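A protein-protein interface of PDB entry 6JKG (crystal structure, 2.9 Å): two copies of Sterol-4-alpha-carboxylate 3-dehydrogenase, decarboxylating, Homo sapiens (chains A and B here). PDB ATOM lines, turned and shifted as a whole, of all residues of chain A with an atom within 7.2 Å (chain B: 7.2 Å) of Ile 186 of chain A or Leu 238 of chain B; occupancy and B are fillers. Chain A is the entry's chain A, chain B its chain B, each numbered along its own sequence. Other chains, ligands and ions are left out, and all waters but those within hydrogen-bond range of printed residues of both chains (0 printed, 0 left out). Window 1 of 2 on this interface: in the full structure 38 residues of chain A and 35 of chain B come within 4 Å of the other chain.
The backbone NH (N) of Ile 184 of chain A is in hydrogen-bond range of the backbone carbonyl oxygen (O) of Val 197 of chain B.
The backbone NH (N) of Leu 238 of chain B is in hydrogen-bond range of the backbone carbonyl oxygen (O) of Ile 184 of chain A, at 2.8 Å.
The backbone carbonyl oxygen (O) of Leu 185 of chain A sits at hydrogen-bond distance from the backbone NH (N) of Val 197 of chain B (2.7 Å).
The backbone NH of Ile 186 of chain A is in hydrogen-bond range of the backbone carbonyl oxygen of His 236 of chain B (2.9 Å).
The backbone NH (N) of Glu 187 of chain A is in hydrogen-bond range of the backbone carbonyl oxygen (O) of Lys 195 of chain B (3.0 Å).
The backbone carbonyl oxygen (O) of Ala 234 of chain B sits at hydrogen-bond distance from the backbone NH (N) of Ala 188 of chain A, 3.3 Å away.
N of His 236 of chain A lies within hydrogen-bond range of O of Ile 186 of chain B (3.0 Å).
O of Ile 237 of chain A is in hydrogen-bond range of N of Glu 239 of chain B (3.2 Å).
OE1 of Glu 239 of chain A is in hydrogen-bond range of ND2 of Asn 212 of chain B (3.4 Å).
The backbone NH (N) of Glu 239 of chain A lies within hydrogen-bond range of the backbone carbonyl oxygen (O) of Ile 237 of chain B, at 3.4 Å.
OE2 of Glu 239 of chain A lies close to O of Leu 238 of chain B.
The backbone carbonyl oxygen (O) of Phe 235 of chain A is in hydrogen-bond range of the backbone NH (N) of Arg 169 of chain A.
The backbone NH (N) of Ala 189 of chain A lies close to the side-chain sulfur (SD) of Met 194 of chain A (3.7 Å).
SD of Met 194 of chain B lies within hydrogen-bond range of N of Ala 189 of chain B (3.1 Å).
The side-chain amide oxygen (OD1) of Asn 212 of chain B sits at hydrogen-bond distance from a ring nitrogen (NE2) of His 240 of chain B (3.0 Å).
Among the printed residues, merely in contact across the chains: Ile 186 of chain A with Ile 186 of chain B, Leu 185 of chain A with Phe 196 of chain B, Leu 185 of chain A with His 236 of chain B, Pro 183 of chain A with Leu 238 of chain B, Phe 235 of chain A with Ile 186 of chain B, Arg 169 of chain A with Ala 188 of chain B, Leu 238 of chain A with Ile 237 of chain B, Phe 235 of chain A with Glu 187 of chain B, Ile 184 of chain A with Ile 237 of chain B, Ala 188 of chain A with His 236 of chain B, Pro 183 of chain A with Val 197 of chain B, Ile 119 of chain A with Phe 196 of chain B, His 236 of chain A with Leu 238 of chain B, Leu 238 of chain A with Ile 186 of chain B, Val 182 of chain A with His 240 of chain B, Glu 239 of chain A with Glu 239 of chain B, Ile 186 of chain A with Phe 235 of chain B, Glu 187 of chain A with Phe 235 of chain B, Glu 187 of chain A with Ala 234 of chain B, Leu 238 of chain A with His 236 of chain B, Ile 184 of chain A with His 240 of chain B, Ile 186 of chain A with Leu 238 of chain B, Ile 237 of chain A with Leu 238 of chain B, His 236 of chain A with Ala 188 of chain B, Met 194 of chain A with Glu 187 of chain B, Leu 185 of chain A with Ile 237 of chain B, Met 194 of chain A with Met 194 of chain B, Ile 186 of chain A with Lys 195 of chain B and Leu 185 of chain A with Phe 235 of chain B.
Ile 186 of chain A touches five residues of chain B.
Printed residues of chain A within 4 Å of Leu 238 of chain B: Pro 183 (3.2 Å), Ile 184 (2.8 Å), Ile 186 (3.8 Å), His 236 (3.5 Å), Ile 237 (3.8 Å) and Glu 239 (3.0 Å).
Of the printed residues of chain A, Phe 196 of chain B touches Ile 119 (3.5 Å) and Leu 185 (3.1 Å).
Printed residues of chain A within 4 Å of Ala 234 of chain B: Glu 187 and Ala 188.
Of the printed residues of chain A, Phe 235 of chain B touches Leu 185 (3.99 Å), Ile 186 (3.6 Å) and Glu 187 (3.6 Å).
Printed residues of chain A within 4 Å of Glu 187 of chain B: Met 194 and Phe 235.
Of the printed residues of chain B, Ile 119 of chain A touches Phe 196 (3.5 Å).
Ala 116 of chain A touches none of the printed residues of chain B.
The nearest residue of chain A that does not touch Leu 238 of chain B is Leu 185 of chain A (4.5 Å).
Hydrophobic or aromatic side chains of chain A that line the printed part of chain B: Ile 119, Val 182, Pro 183, Ile 184, Leu 185, Ile 186, Ala 188, Met 194, Phe 235, His 236, Ile 237 and Leu 238.
Printed residues of chain B that touch a printed residue of chain A: Ile 186, Glu 187, Ala 188, Met 194, Lys 195, Phe 196, Val 197, Asn 212, Ala 234, Phe 235, His 236, Ile 237, Leu 238, Glu 239 and His 240.
Hydrophobic or aromatic side chains of chain B within 4 Å of the printed part of chain A: Ile 186, Ala 188, Met 194, Phe 196, Val 197, Phe 235, His 236, Ile 237, Leu 238 and His 240.
Among the printed residues, 40 pairs touch across the chains.
Ile 186 of chain A touches Leu 238 of chain B, and with the chains exchanged Leu 238 of chain A touches Ile 186 of chain B.
Met 194 of chain A touches Glu 187 of chain B, but with the chains exchanged Glu 187 of chain A does not touch Met 194 of chain B (4.1 Å).
Met 194 of chain A touches its own counterpart, Met 194 of chain B.
Glu 239 of chain A touches Leu 238 of chain B, but with the chains exchanged Leu 238 of chain A does not touch Glu 239 of chain B (4.6 Å).
10 positions are printed for both chains.
Of the 40 pairs that touch across the chains among the printed residues, 19 have their exchanged pair printed and touching as well.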
ATOM      1  N   ALA A 116     -10.298  18.505 -29.628  1.00  0.00           N
ATOM      2  CA  ALA A 116     -10.675  17.396 -28.753  1.00  0.00           C
ATOM      3  C   ALA A 116     -11.282  16.220 -29.523  1.00  0.00           C
ATOM      4  O   ALA A 116     -11.143  15.061 -29.110  1.00  0.00           O
ATOM      5  CB  ALA A 116     -11.644  17.894 -27.683  1.00  0.00           C
ATOM      6  N   ILE A 119      -9.717  12.592 -30.936  1.00  0.00           N
ATOM      7  CA  ILE A 119      -9.614  11.378 -30.088  1.00  0.00           C
ATOM      8  C   ILE A 119     -10.487  10.297 -30.708  1.00  0.00           C
ATOM      9  O   ILE A 119     -10.286   9.150 -30.385  1.00  0.00           O
ATOM     10  CB  ILE A 119     -10.078  11.711 -28.662  1.00  0.00           C
ATOM     11  CG1 ILE A 119      -9.331  10.892 -27.612  1.00  0.00           C
ATOM     12  CG2 ILE A 119     -11.571  11.526 -28.536  1.00  0.00           C
ATOM     13  CD1 ILE A 119      -9.918  10.980 -26.225  1.00  0.00           C
ATOM     14  N   ARG A 169      -5.737  20.176 -27.124  1.00  0.00           N
ATOM     15  CA  ARG A 169      -6.991  19.778 -27.779  1.00  0.00           C
ATOM     16  C   ARG A 169      -8.188  20.430 -27.099  1.00  0.00           C
ATOM     17  O   ARG A 169      -8.839  19.802 -26.247  1.00  0.00           O
ATOM     18  CB  ARG A 169      -7.175  18.259 -27.776  1.00  0.00           C
ATOM     19  CG  ARG A 169      -6.317  17.475 -28.742  1.00  0.00           C
ATOM     20  CD  ARG A 169      -6.082  16.068 -28.222  1.00  0.00           C
ATOM     21  NE  ARG A 169      -5.233  15.298 -29.123  1.00  0.00           N
ATOM     22  CZ  ARG A 169      -5.017  13.985 -29.042  1.00  0.00           C
ATOM     23  NH1 ARG A 169      -5.583  13.254 -28.080  1.00  0.00           N
ATOM     24  NH2 ARG A 169      -4.214  13.400 -29.925  1.00  0.00           N
ATOM     25  N   VAL A 182     -18.893  14.050 -28.051  1.00  0.00           N
ATOM     26  CA  VAL A 182     -17.976  14.799 -27.191  1.00  0.00           C
ATOM     27  C   VAL A 182     -17.400  13.888 -26.109  1.00  0.00           C
ATOM     28  O   VAL A 182     -18.131  13.083 -25.519  1.00  0.00           O
ATOM     29  CB  VAL A 182     -18.689  16.018 -26.585  1.00  0.00           C
ATOM     30  CG1 VAL A 182     -20.023  15.601 -26.011  1.00  0.00           C
ATOM     31  CG2 VAL A 182     -17.835  16.676 -25.522  1.00  0.00           C
ATOM     32  N   PRO A 183     -16.098  13.962 -25.832  1.00  0.00           N
ATOM     33  CA  PRO A 183     -15.509  13.130 -24.766  1.00  0.00           C
ATOM     34  C   PRO A 183     -15.660  13.785 -23.398  1.00  0.00           C
ATOM     35  O   PRO A 183     -15.134  14.874 -23.143  1.00  0.00           O
ATOM     36  CB  PRO A 183     -14.041  13.007 -25.184  1.00  0.00           C
ATOM     37  CG  PRO A 183     -13.790  14.148 -26.098  1.00  0.00           C
ATOM     38  CD  PRO A 183     -15.081  14.633 -26.658  1.00  0.00           C
ATOM     39  N   ILE A 184     -16.379  13.102 -22.509  1.00  0.00           N
ATOM     40  CA  ILE A 184     -16.713  13.665 -21.203  1.00  0.00           C
ATOM     41  C   ILE A 184     -15.705  13.241 -20.143  1.00  0.00           C
ATOM     42  O   ILE A 184     -15.386  14.009 -19.231  1.00  0.00           O
ATOM     43  CB  ILE A 184     -18.155  13.270 -20.804  1.00  0.00           C
ATOM     44  CG1 ILE A 184     -19.138  13.449 -21.969  1.00  0.00           C
ATOM     45  CG2 ILE A 184     -18.632  14.116 -19.631  1.00  0.00           C
ATOM     46  CD1 ILE A 184     -19.333  14.866 -22.405  1.00  0.00           C
ATOM     47  N   LEU A 185     -15.179  12.022 -20.255  1.00  0.00           N
ATOM     48  CA  LEU A 185     -14.290  11.453 -19.253  1.00  0.00           C
ATOM     49  C   LEU A 185     -13.113  10.763 -19.921  1.00  0.00           C
ATOM     50  O   LEU A 185     -13.274  10.119 -20.961  1.00  0.00           O
ATOM     51  CB  LEU A 185     -15.026  10.438 -18.371  1.00  0.00           C
ATOM     52  CG  LEU A 185     -16.337  10.882 -17.731  1.00  0.00           C
ATOM     53  CD1 LEU A 185     -17.020   9.672 -17.149  1.00  0.00           C
ATOM     54  CD2 LEU A 185     -16.104  11.953 -16.664  1.00  0.00           C
ATOM     55  N   ILE A 186     -11.939  10.868 -19.297  1.00  0.00           N
ATOM     56  CA  ILE A 186     -10.705  10.289 -19.825  1.00  0.00           C
ATOM     57  C   ILE A 186      -9.996   9.527 -18.710  1.00  0.00           C
ATOM     58  O   ILE A 186      -9.826  10.048 -17.601  1.00  0.00           O
ATOM     59  CB  ILE A 186      -9.778  11.363 -20.429  1.00  0.00           C
ATOM     60  CG1 ILE A 186      -8.487  10.713 -20.942  1.00  0.00           C
ATOM     61  CG2 ILE A 186      -9.525  12.483 -19.429  1.00  0.00           C
ATOM     62  CD1 ILE A 186      -7.569  11.648 -21.698  1.00  0.00           C
ATOM     63  N   GLU A 187      -9.592   8.292 -19.009  1.00  0.00           N
ATOM     64  CA  GLU A 187      -9.040   7.410 -17.990  1.00  0.00           C
ATOM     65  C   GLU A 187      -7.748   7.986 -17.445  1.00  0.00           C
ATOM     66  O   GLU A 187      -6.872   8.407 -18.208  1.00  0.00           O
ATOM     67  CB  GLU A 187      -8.782   6.011 -18.559  1.00  0.00           C
ATOM     68  CG  GLU A 187      -7.584   5.310 -17.905  1.00  0.00           C
ATOM     69  CD  GLU A 187      -7.449   3.832 -18.263  1.00  0.00           C
ATOM     70  OE1 GLU A 187      -8.035   3.403 -19.284  1.00  0.00           O
ATOM     71  OE2 GLU A 187      -6.740   3.106 -17.521  1.00  0.00           O
ATOM     72  N   ALA A 188      -7.630   8.015 -16.128  1.00  0.00           N
ATOM     73  CA  ALA A 188      -6.369   8.466 -15.530  1.00  0.00           C
ATOM     74  C   ALA A 188      -5.514   7.219 -15.443  1.00  0.00           C
ATOM     75  O   ALA A 188      -6.036   6.209 -15.023  1.00  0.00           O
ATOM     76  CB  ALA A 188      -6.631   9.025 -14.179  1.00  0.00           C
ATOM     77  N   ALA A 189      -4.240   7.305 -15.802  1.00  0.00           N
ATOM     78  CA  ALA A 189      -3.383   6.103 -15.840  1.00  0.00           C
ATOM     79  C   ALA A 189      -3.001   5.622 -14.444  1.00  0.00           C
ATOM     80  O   ALA A 189      -3.103   6.403 -13.488  1.00  0.00           O
ATOM     81  CB  ALA A 189      -2.154   6.377 -16.657  1.00  0.00           C
ATOM     82  N   MET A 194       1.027   9.406 -17.830  1.00  0.00           N
ATOM     83  CA  MET A 194       0.118  10.518 -18.080  1.00  0.00           C
ATOM     84  C   MET A 194       0.790  11.747 -17.497  1.00  0.00           C
ATOM     85  O   MET A 194       1.036  11.762 -16.303  1.00  0.00           O
ATOM     86  CB  MET A 194      -1.150  10.266 -17.281  1.00  0.00           C
ATOM     87  CG  MET A 194      -2.188  11.311 -17.515  1.00  0.00           C
ATOM     88  SD  MET A 194      -3.650  10.834 -16.618  1.00  0.00           S
ATOM     89  CE  MET A 194      -4.307   9.579 -17.712  1.00  0.00           C
ATOM     90  N   PHE A 235      -2.658  16.953 -25.319  1.00  0.00           N
ATOM     91  CA  PHE A 235      -3.301  17.231 -24.048  1.00  0.00           C
ATOM     92  C   PHE A 235      -4.766  17.608 -24.242  1.00  0.00           C
ATOM     93  O   PHE A 235      -5.146  18.213 -25.253  1.00  0.00           O
ATOM     94  CB  PHE A 235      -2.586  18.335 -23.293  1.00  0.00           C
ATOM     95  CG  PHE A 235      -1.332  17.882 -22.615  1.00  0.00           C
ATOM     96  CD1 PHE A 235      -0.133  17.752 -23.322  1.00  0.00           C
ATOM     97  CD2 PHE A 235      -1.331  17.602 -21.261  1.00  0.00           C
ATOM     98  CE1 PHE A 235       1.033  17.337 -22.685  1.00  0.00           C
ATOM     99  CE2 PHE A 235      -0.165  17.195 -20.619  1.00  0.00           C
ATOM    100  CZ  PHE A 235       1.016  17.058 -21.335  1.00  0.00           C
ATOM    101  N   HIS A 236      -5.582  17.224 -23.260  1.00  0.00           N
ATOM    102  CA  HIS A 236      -6.942  17.710 -23.124  1.00  0.00           C
ATOM    103  C   HIS A 236      -7.008  18.699 -21.964  1.00  0.00           C
ATOM    104  O   HIS A 236      -6.051  18.843 -21.191  1.00  0.00           O
ATOM    105  CB  HIS A 236      -7.911  16.545 -22.920  1.00  0.00           C
ATOM    106  CG  HIS A 236      -8.219  15.806 -24.183  1.00  0.00           C
ATOM    107  ND1 HIS A 236      -9.505  15.659 -24.674  1.00  0.00           N
ATOM    108  CD2 HIS A 236      -7.401  15.221 -25.090  1.00  0.00           C
ATOM    109  CE1 HIS A 236      -9.464  14.993 -25.817  1.00  0.00           C
ATOM    110  NE2 HIS A 236      -8.200  14.716 -26.092  1.00  0.00           N
ATOM    111  N   ILE A 237      -8.148  19.386 -21.861  1.00  0.00           N
ATOM    112  CA  ILE A 237      -8.378  20.406 -20.845  1.00  0.00           C
ATOM    113  C   ILE A 237      -9.412  19.923 -19.832  1.00  0.00           C
ATOM    114  O   ILE A 237     -10.576  19.672 -20.184  1.00  0.00           O
ATOM    115  CB  ILE A 237      -8.848  21.719 -21.481  1.00  0.00           C
ATOM    116  CG1 ILE A 237      -7.952  22.106 -22.666  1.00  0.00           C
ATOM    117  CG2 ILE A 237      -8.916  22.802 -20.417  1.00  0.00           C
ATOM    118  CD1 ILE A 237      -8.473  23.285 -23.470  1.00  0.00           C
ATOM    119  N   LEU A 238      -9.001  19.845 -18.568  1.00  0.00           N
ATOM    120  CA  LEU A 238      -9.873  19.479 -17.460  1.00  0.00           C
ATOM    121  C   LEU A 238     -10.904  20.572 -17.175  1.00  0.00           C
ATOM    122  O   LEU A 238     -10.747  21.738 -17.551  1.00  0.00           O
ATOM    123  CB  LEU A 238      -9.058  19.207 -16.194  1.00  0.00           C
ATOM    124  CG  LEU A 238      -8.067  18.064 -16.318  1.00  0.00           C
ATOM    125  CD1 LEU A 238      -7.461  17.737 -14.983  1.00  0.00           C
ATOM    126  CD2 LEU A 238      -8.838  16.876 -16.823  1.00  0.00           C
ATOM    127  N   GLU A 239     -11.963  20.166 -16.468  1.00  0.00           N
ATOM    128  CA  GLU A 239     -13.033  21.041 -16.019  1.00  0.00           C
ATOM    129  C   GLU A 239     -12.751  21.586 -14.625  1.00  0.00           C
ATOM    130  O   GLU A 239     -12.179  20.902 -13.771  1.00  0.00           O
ATOM    131  CB  GLU A 239     -14.353  20.289 -16.019  1.00  0.00           C
ATOM    132  CG  GLU A 239     -15.055  20.360 -17.325  1.00  0.00           C
ATOM    133  CD  GLU A 239     -16.542  20.318 -17.146  1.00  0.00           C
ATOM    134  OE1 GLU A 239     -17.115  21.330 -16.681  1.00  0.00           O
ATOM    135  OE2 GLU A 239     -17.134  19.270 -17.475  1.00  0.00           O
ATOM    136  N   ILE B 186      -4.246  17.082 -19.269  1.00  0.00           N
ATOM    137  CA  ILE B 186      -3.781  15.709 -19.102  1.00  0.00           C
ATOM    138  C   ILE B 186      -3.377  15.153 -20.460  1.00  0.00           C
ATOM    139  O   ILE B 186      -4.073  15.361 -21.461  1.00  0.00           O
ATOM    140  CB  ILE B 186      -4.825  14.796 -18.411  1.00  0.00           C
ATOM    141  CG1 ILE B 186      -5.792  14.155 -19.405  1.00  0.00           C
ATOM    142  CG2 ILE B 186      -5.615  15.532 -17.342  1.00  0.00           C
ATOM    143  CD1 ILE B 186      -6.723  13.164 -18.767  1.00  0.00           C
ATOM    144  N   GLU B 187      -2.239  14.469 -20.491  1.00  0.00           N
ATOM    145  CA  GLU B 187      -1.812  13.768 -21.689  1.00  0.00           C
ATOM    146  C   GLU B 187      -2.874  12.775 -22.132  1.00  0.00           C
ATOM    147  O   GLU B 187      -3.440  12.043 -21.318  1.00  0.00           O
ATOM    148  CB  GLU B 187      -0.503  13.031 -21.428  1.00  0.00           C
ATOM    149  CG  GLU B 187      -0.097  12.099 -22.551  1.00  0.00           C
ATOM    150  CD  GLU B 187       1.165  11.306 -22.229  1.00  0.00           C
ATOM    151  OE1 GLU B 187       1.893  11.674 -21.275  1.00  0.00           O
ATOM    152  OE2 GLU B 187       1.426  10.307 -22.933  1.00  0.00           O
ATOM    153  N   ALA B 188      -3.151  12.752 -23.433  1.00  0.00           N
ATOM    154  CA  ALA B 188      -3.935  11.685 -24.047  1.00  0.00           C
ATOM    155  C   ALA B 188      -2.971  10.784 -24.804  1.00  0.00           C
ATOM    156  O   ALA B 188      -2.473  11.168 -25.869  1.00  0.00           O
ATOM    157  CB  ALA B 188      -5.008  12.245 -24.978  1.00  0.00           C
ATOM    158  N   ALA B 189      -2.705   9.597 -24.249  1.00  0.00           N
ATOM    159  CA  ALA B 189      -1.787   8.645 -24.871  1.00  0.00           C
ATOM    160  C   ALA B 189      -2.098   8.481 -26.352  1.00  0.00           C
ATOM    161  O   ALA B 189      -3.260   8.340 -26.744  1.00  0.00           O
ATOM    162  CB  ALA B 189      -1.866   7.289 -24.170  1.00  0.00           C
ATOM    163  N   MET B 194      -5.609   4.706 -23.856  1.00  0.00           N
ATOM    164  CA  MET B 194      -6.536   5.212 -22.852  1.00  0.00           C
ATOM    165  C   MET B 194      -7.980   5.073 -23.327  1.00  0.00           C
ATOM    166  O   MET B 194      -8.317   5.392 -24.471  1.00  0.00           O
ATOM    167  CB  MET B 194      -6.239   6.683 -22.536  1.00  0.00           C
ATOM    168  CG  MET B 194      -5.060   6.927 -21.596  1.00  0.00           C
ATOM    169  SD  MET B 194      -4.312   8.565 -21.804  1.00  0.00           S
ATOM    170  CE  MET B 194      -2.737   8.313 -20.999  1.00  0.00           C
ATOM    171  N   LYS B 195      -8.837   4.584 -22.433  1.00  0.00           N
ATOM    172  CA  LYS B 195     -10.270   4.592 -22.685  1.00  0.00           C
ATOM    173  C   LYS B 195     -10.863   5.947 -22.307  1.00  0.00           C
ATOM    174  O   LYS B 195     -10.347   6.670 -21.454  1.00  0.00           O
ATOM    175  CB  LYS B 195     -10.969   3.482 -21.896  1.00  0.00           C
ATOM    176  CG  LYS B 195     -10.827   2.093 -22.496  1.00  0.00           C
ATOM    177  CD  LYS B 195     -10.647   1.044 -21.411  1.00  0.00           C
ATOM    178  CE  LYS B 195     -10.293  -0.310 -22.010  1.00  0.00           C
ATOM    179  NZ  LYS B 195      -9.321  -0.195 -23.131  1.00  0.00           N
ATOM    180  N   PHE B 196     -11.967   6.291 -22.951  1.00  0.00           N
ATOM    181  CA  PHE B 196     -12.606   7.556 -22.633  1.00  0.00           C
ATOM    182  C   PHE B 196     -14.104   7.405 -22.820  1.00  0.00           C
ATOM    183  O   PHE B 196     -14.564   6.584 -23.616  1.00  0.00           O
ATOM    184  CB  PHE B 196     -12.056   8.721 -23.487  1.00  0.00           C
ATOM    185  CG  PHE B 196     -12.124   8.483 -24.978  1.00  0.00           C
ATOM    186  CD1 PHE B 196     -11.125   7.772 -25.633  1.00  0.00           C
ATOM    187  CD2 PHE B 196     -13.193   8.968 -25.724  1.00  0.00           C
ATOM    188  CE1 PHE B 196     -11.189   7.551 -27.001  1.00  0.00           C
ATOM    189  CE2 PHE B 196     -13.266   8.748 -27.091  1.00  0.00           C
ATOM    190  CZ  PHE B 196     -12.262   8.038 -27.731  1.00  0.00           C
ATOM    191  N   VAL B 197     -14.863   8.200 -22.084  1.00  0.00           N
ATOM    192  CA  VAL B 197     -16.316   8.104 -22.074  1.00  0.00           C
ATOM    193  C   VAL B 197     -16.885   9.170 -23.001  1.00  0.00           C
ATOM    194  O   VAL B 197     -16.479  10.338 -22.941  1.00  0.00           O
ATOM    195  CB  VAL B 197     -16.862   8.239 -20.643  1.00  0.00           C
ATOM    196  CG1 VAL B 197     -18.360   8.468 -20.654  1.00  0.00           C
ATOM    197  CG2 VAL B 197     -16.516   6.994 -19.848  1.00  0.00           C
ATOM    198  N   ASN B 212     -21.997  19.339 -14.782  1.00  0.00           N
ATOM    199  CA  ASN B 212     -21.157  18.510 -15.638  1.00  0.00           C
ATOM    200  C   ASN B 212     -20.430  17.455 -14.823  1.00  0.00           C
ATOM    201  O   ASN B 212     -20.165  16.353 -15.313  1.00  0.00           O
ATOM    202  CB  ASN B 212     -20.172  19.389 -16.399  1.00  0.00           C
ATOM    203  CG  ASN B 212     -20.855  20.244 -17.441  1.00  0.00           C
ATOM    204  OD1 ASN B 212     -21.814  19.809 -18.077  1.00  0.00           O
ATOM    205  ND2 ASN B 212     -20.359  21.460 -17.633  1.00  0.00           N
ATOM    206  N   ALA B 234     -10.030   4.968 -12.406  1.00  0.00           N
ATOM    207  CA  ALA B 234     -10.273   6.381 -12.126  1.00  0.00           C
ATOM    208  C   ALA B 234     -10.482   7.142 -13.432  1.00  0.00           C
ATOM    209  O   ALA B 234     -10.135   6.660 -14.510  1.00  0.00           O
ATOM    210  CB  ALA B 234      -9.102   6.984 -11.340  1.00  0.00           C
ATOM    211  N   PHE B 235     -11.079   8.330 -13.337  1.00  0.00           N
ATOM    212  CA  PHE B 235     -11.461   9.087 -14.527  1.00  0.00           C
ATOM    213  C   PHE B 235     -11.480  10.583 -14.249  1.00  0.00           C
ATOM    214  O   PHE B 235     -12.152  11.034 -13.313  1.00  0.00           O
ATOM    215  CB  PHE B 235     -12.851   8.694 -15.042  1.00  0.00           C
ATOM    216  CG  PHE B 235     -12.886   7.429 -15.859  1.00  0.00           C
ATOM    217  CD1 PHE B 235     -12.629   7.457 -17.220  1.00  0.00           C
ATOM    218  CD2 PHE B 235     -13.254   6.222 -15.282  1.00  0.00           C
ATOM    219  CE1 PHE B 235     -12.697   6.291 -17.986  1.00  0.00           C
ATOM    220  CE2 PHE B 235     -13.329   5.063 -16.043  1.00  0.00           C
ATOM    221  CZ  PHE B 235     -13.047   5.100 -17.399  1.00  0.00           C
ATOM    222  N   HIS B 236     -10.785  11.351 -15.094  1.00  0.00           N
ATOM    223  CA  HIS B 236     -10.903  12.804 -15.090  1.00  0.00           C
ATOM    224  C   HIS B 236     -12.037  13.261 -16.009  1.00  0.00           C
ATOM    225  O   HIS B 236     -12.426  12.561 -16.948  1.00  0.00           O
ATOM    226  CB  HIS B 236      -9.592  13.464 -15.522  1.00  0.00           C
ATOM    227  CG  HIS B 236      -8.449  13.220 -14.583  1.00  0.00           C
ATOM    228  ND1 HIS B 236      -8.221  14.000 -13.469  1.00  0.00           N
ATOM    229  CD2 HIS B 236      -7.450  12.305 -14.613  1.00  0.00           C
ATOM    230  CE1 HIS B 236      -7.149  13.557 -12.837  1.00  0.00           C
ATOM    231  NE2 HIS B 236      -6.660  12.533 -13.513  1.00  0.00           N
ATOM    232  N   ILE B 237     -12.556  14.456 -15.737  1.00  0.00           N
ATOM    233  CA  ILE B 237     -13.635  15.047 -16.527  1.00  0.00           C
ATOM    234  C   ILE B 237     -13.049  16.041 -17.525  1.00  0.00           C
ATOM    235  O   ILE B 237     -12.150  16.824 -17.187  1.00  0.00           O
ATOM    236  CB  ILE B 237     -14.673  15.736 -15.625  1.00  0.00           C
ATOM    237  CG1 ILE B 237     -14.991  14.857 -14.413  1.00  0.00           C
ATOM    238  CG2 ILE B 237     -15.925  16.038 -16.418  1.00  0.00           C
ATOM    239  CD1 ILE B 237     -16.125  15.391 -13.547  1.00  0.00           C
ATOM    240  N   LEU B 238     -13.573  16.025 -18.748  1.00  0.00           N
ATOM    241  CA  LEU B 238     -13.150  16.941 -19.797  1.00  0.00           C
ATOM    242  C   LEU B 238     -14.128  18.104 -19.923  1.00  0.00           C
ATOM    243  O   LEU B 238     -15.263  18.037 -19.444  1.00  0.00           O
ATOM    244  CB  LEU B 238     -13.049  16.201 -21.131  1.00  0.00           C
ATOM    245  CG  LEU B 238     -11.983  15.117 -21.148  1.00  0.00           C
ATOM    246  CD1 LEU B 238     -11.955  14.351 -22.452  1.00  0.00           C
ATOM    247  CD2 LEU B 238     -10.649  15.767 -20.887  1.00  0.00           C
ATOM    248  N   GLU B 239     -13.687  19.168 -20.593  1.00  0.00           N
ATOM    249  CA  GLU B 239     -14.609  20.254 -20.886  1.00  0.00           C
ATOM    250  C   GLU B 239     -15.295  20.013 -22.230  1.00  0.00           C
ATOM    251  O   GLU B 239     -14.903  19.148 -23.022  1.00  0.00           O
ATOM    252  CB  GLU B 239     -13.891  21.601 -20.889  1.00  0.00           C
ATOM    253  CG  GLU B 239     -12.619  21.640 -21.709  1.00  0.00           C
ATOM    254  CD  GLU B 239     -12.871  22.040 -23.152  1.00  0.00           C
ATOM    255  OE1 GLU B 239     -13.705  22.942 -23.378  1.00  0.00           O
ATOM    256  OE2 GLU B 239     -12.235  21.461 -24.059  1.00  0.00           O
ATOM    257  N   HIS B 240     -16.352  20.791 -22.473  1.00  0.00           N
ATOM    258  CA  HIS B 240     -17.125  20.730 -23.703  1.00  0.00           C
ATOM    259  C   HIS B 240     -17.690  22.129 -23.958  1.00  0.00           C
ATOM    260  O   HIS B 240     -18.807  22.454 -23.566  1.00  0.00           O
ATOM    261  CB  HIS B 240     -18.208  19.655 -23.622  1.00  0.00           C
ATOM    262  CG  HIS B 240     -18.976  19.674 -22.337  1.00  0.00           C
ATOM    263  ND1 HIS B 240     -19.264  18.528 -21.631  1.00  0.00           N
ATOM    264  CD2 HIS B 240     -19.495  20.699 -21.620  1.00  0.00           C
ATOM    265  CE1 HIS B 240     -19.931  18.843 -20.538  1.00  0.00           C
ATOM    266  NE2 HIS B 240     -20.085  20.154 -20.506  1.00  0.00           N
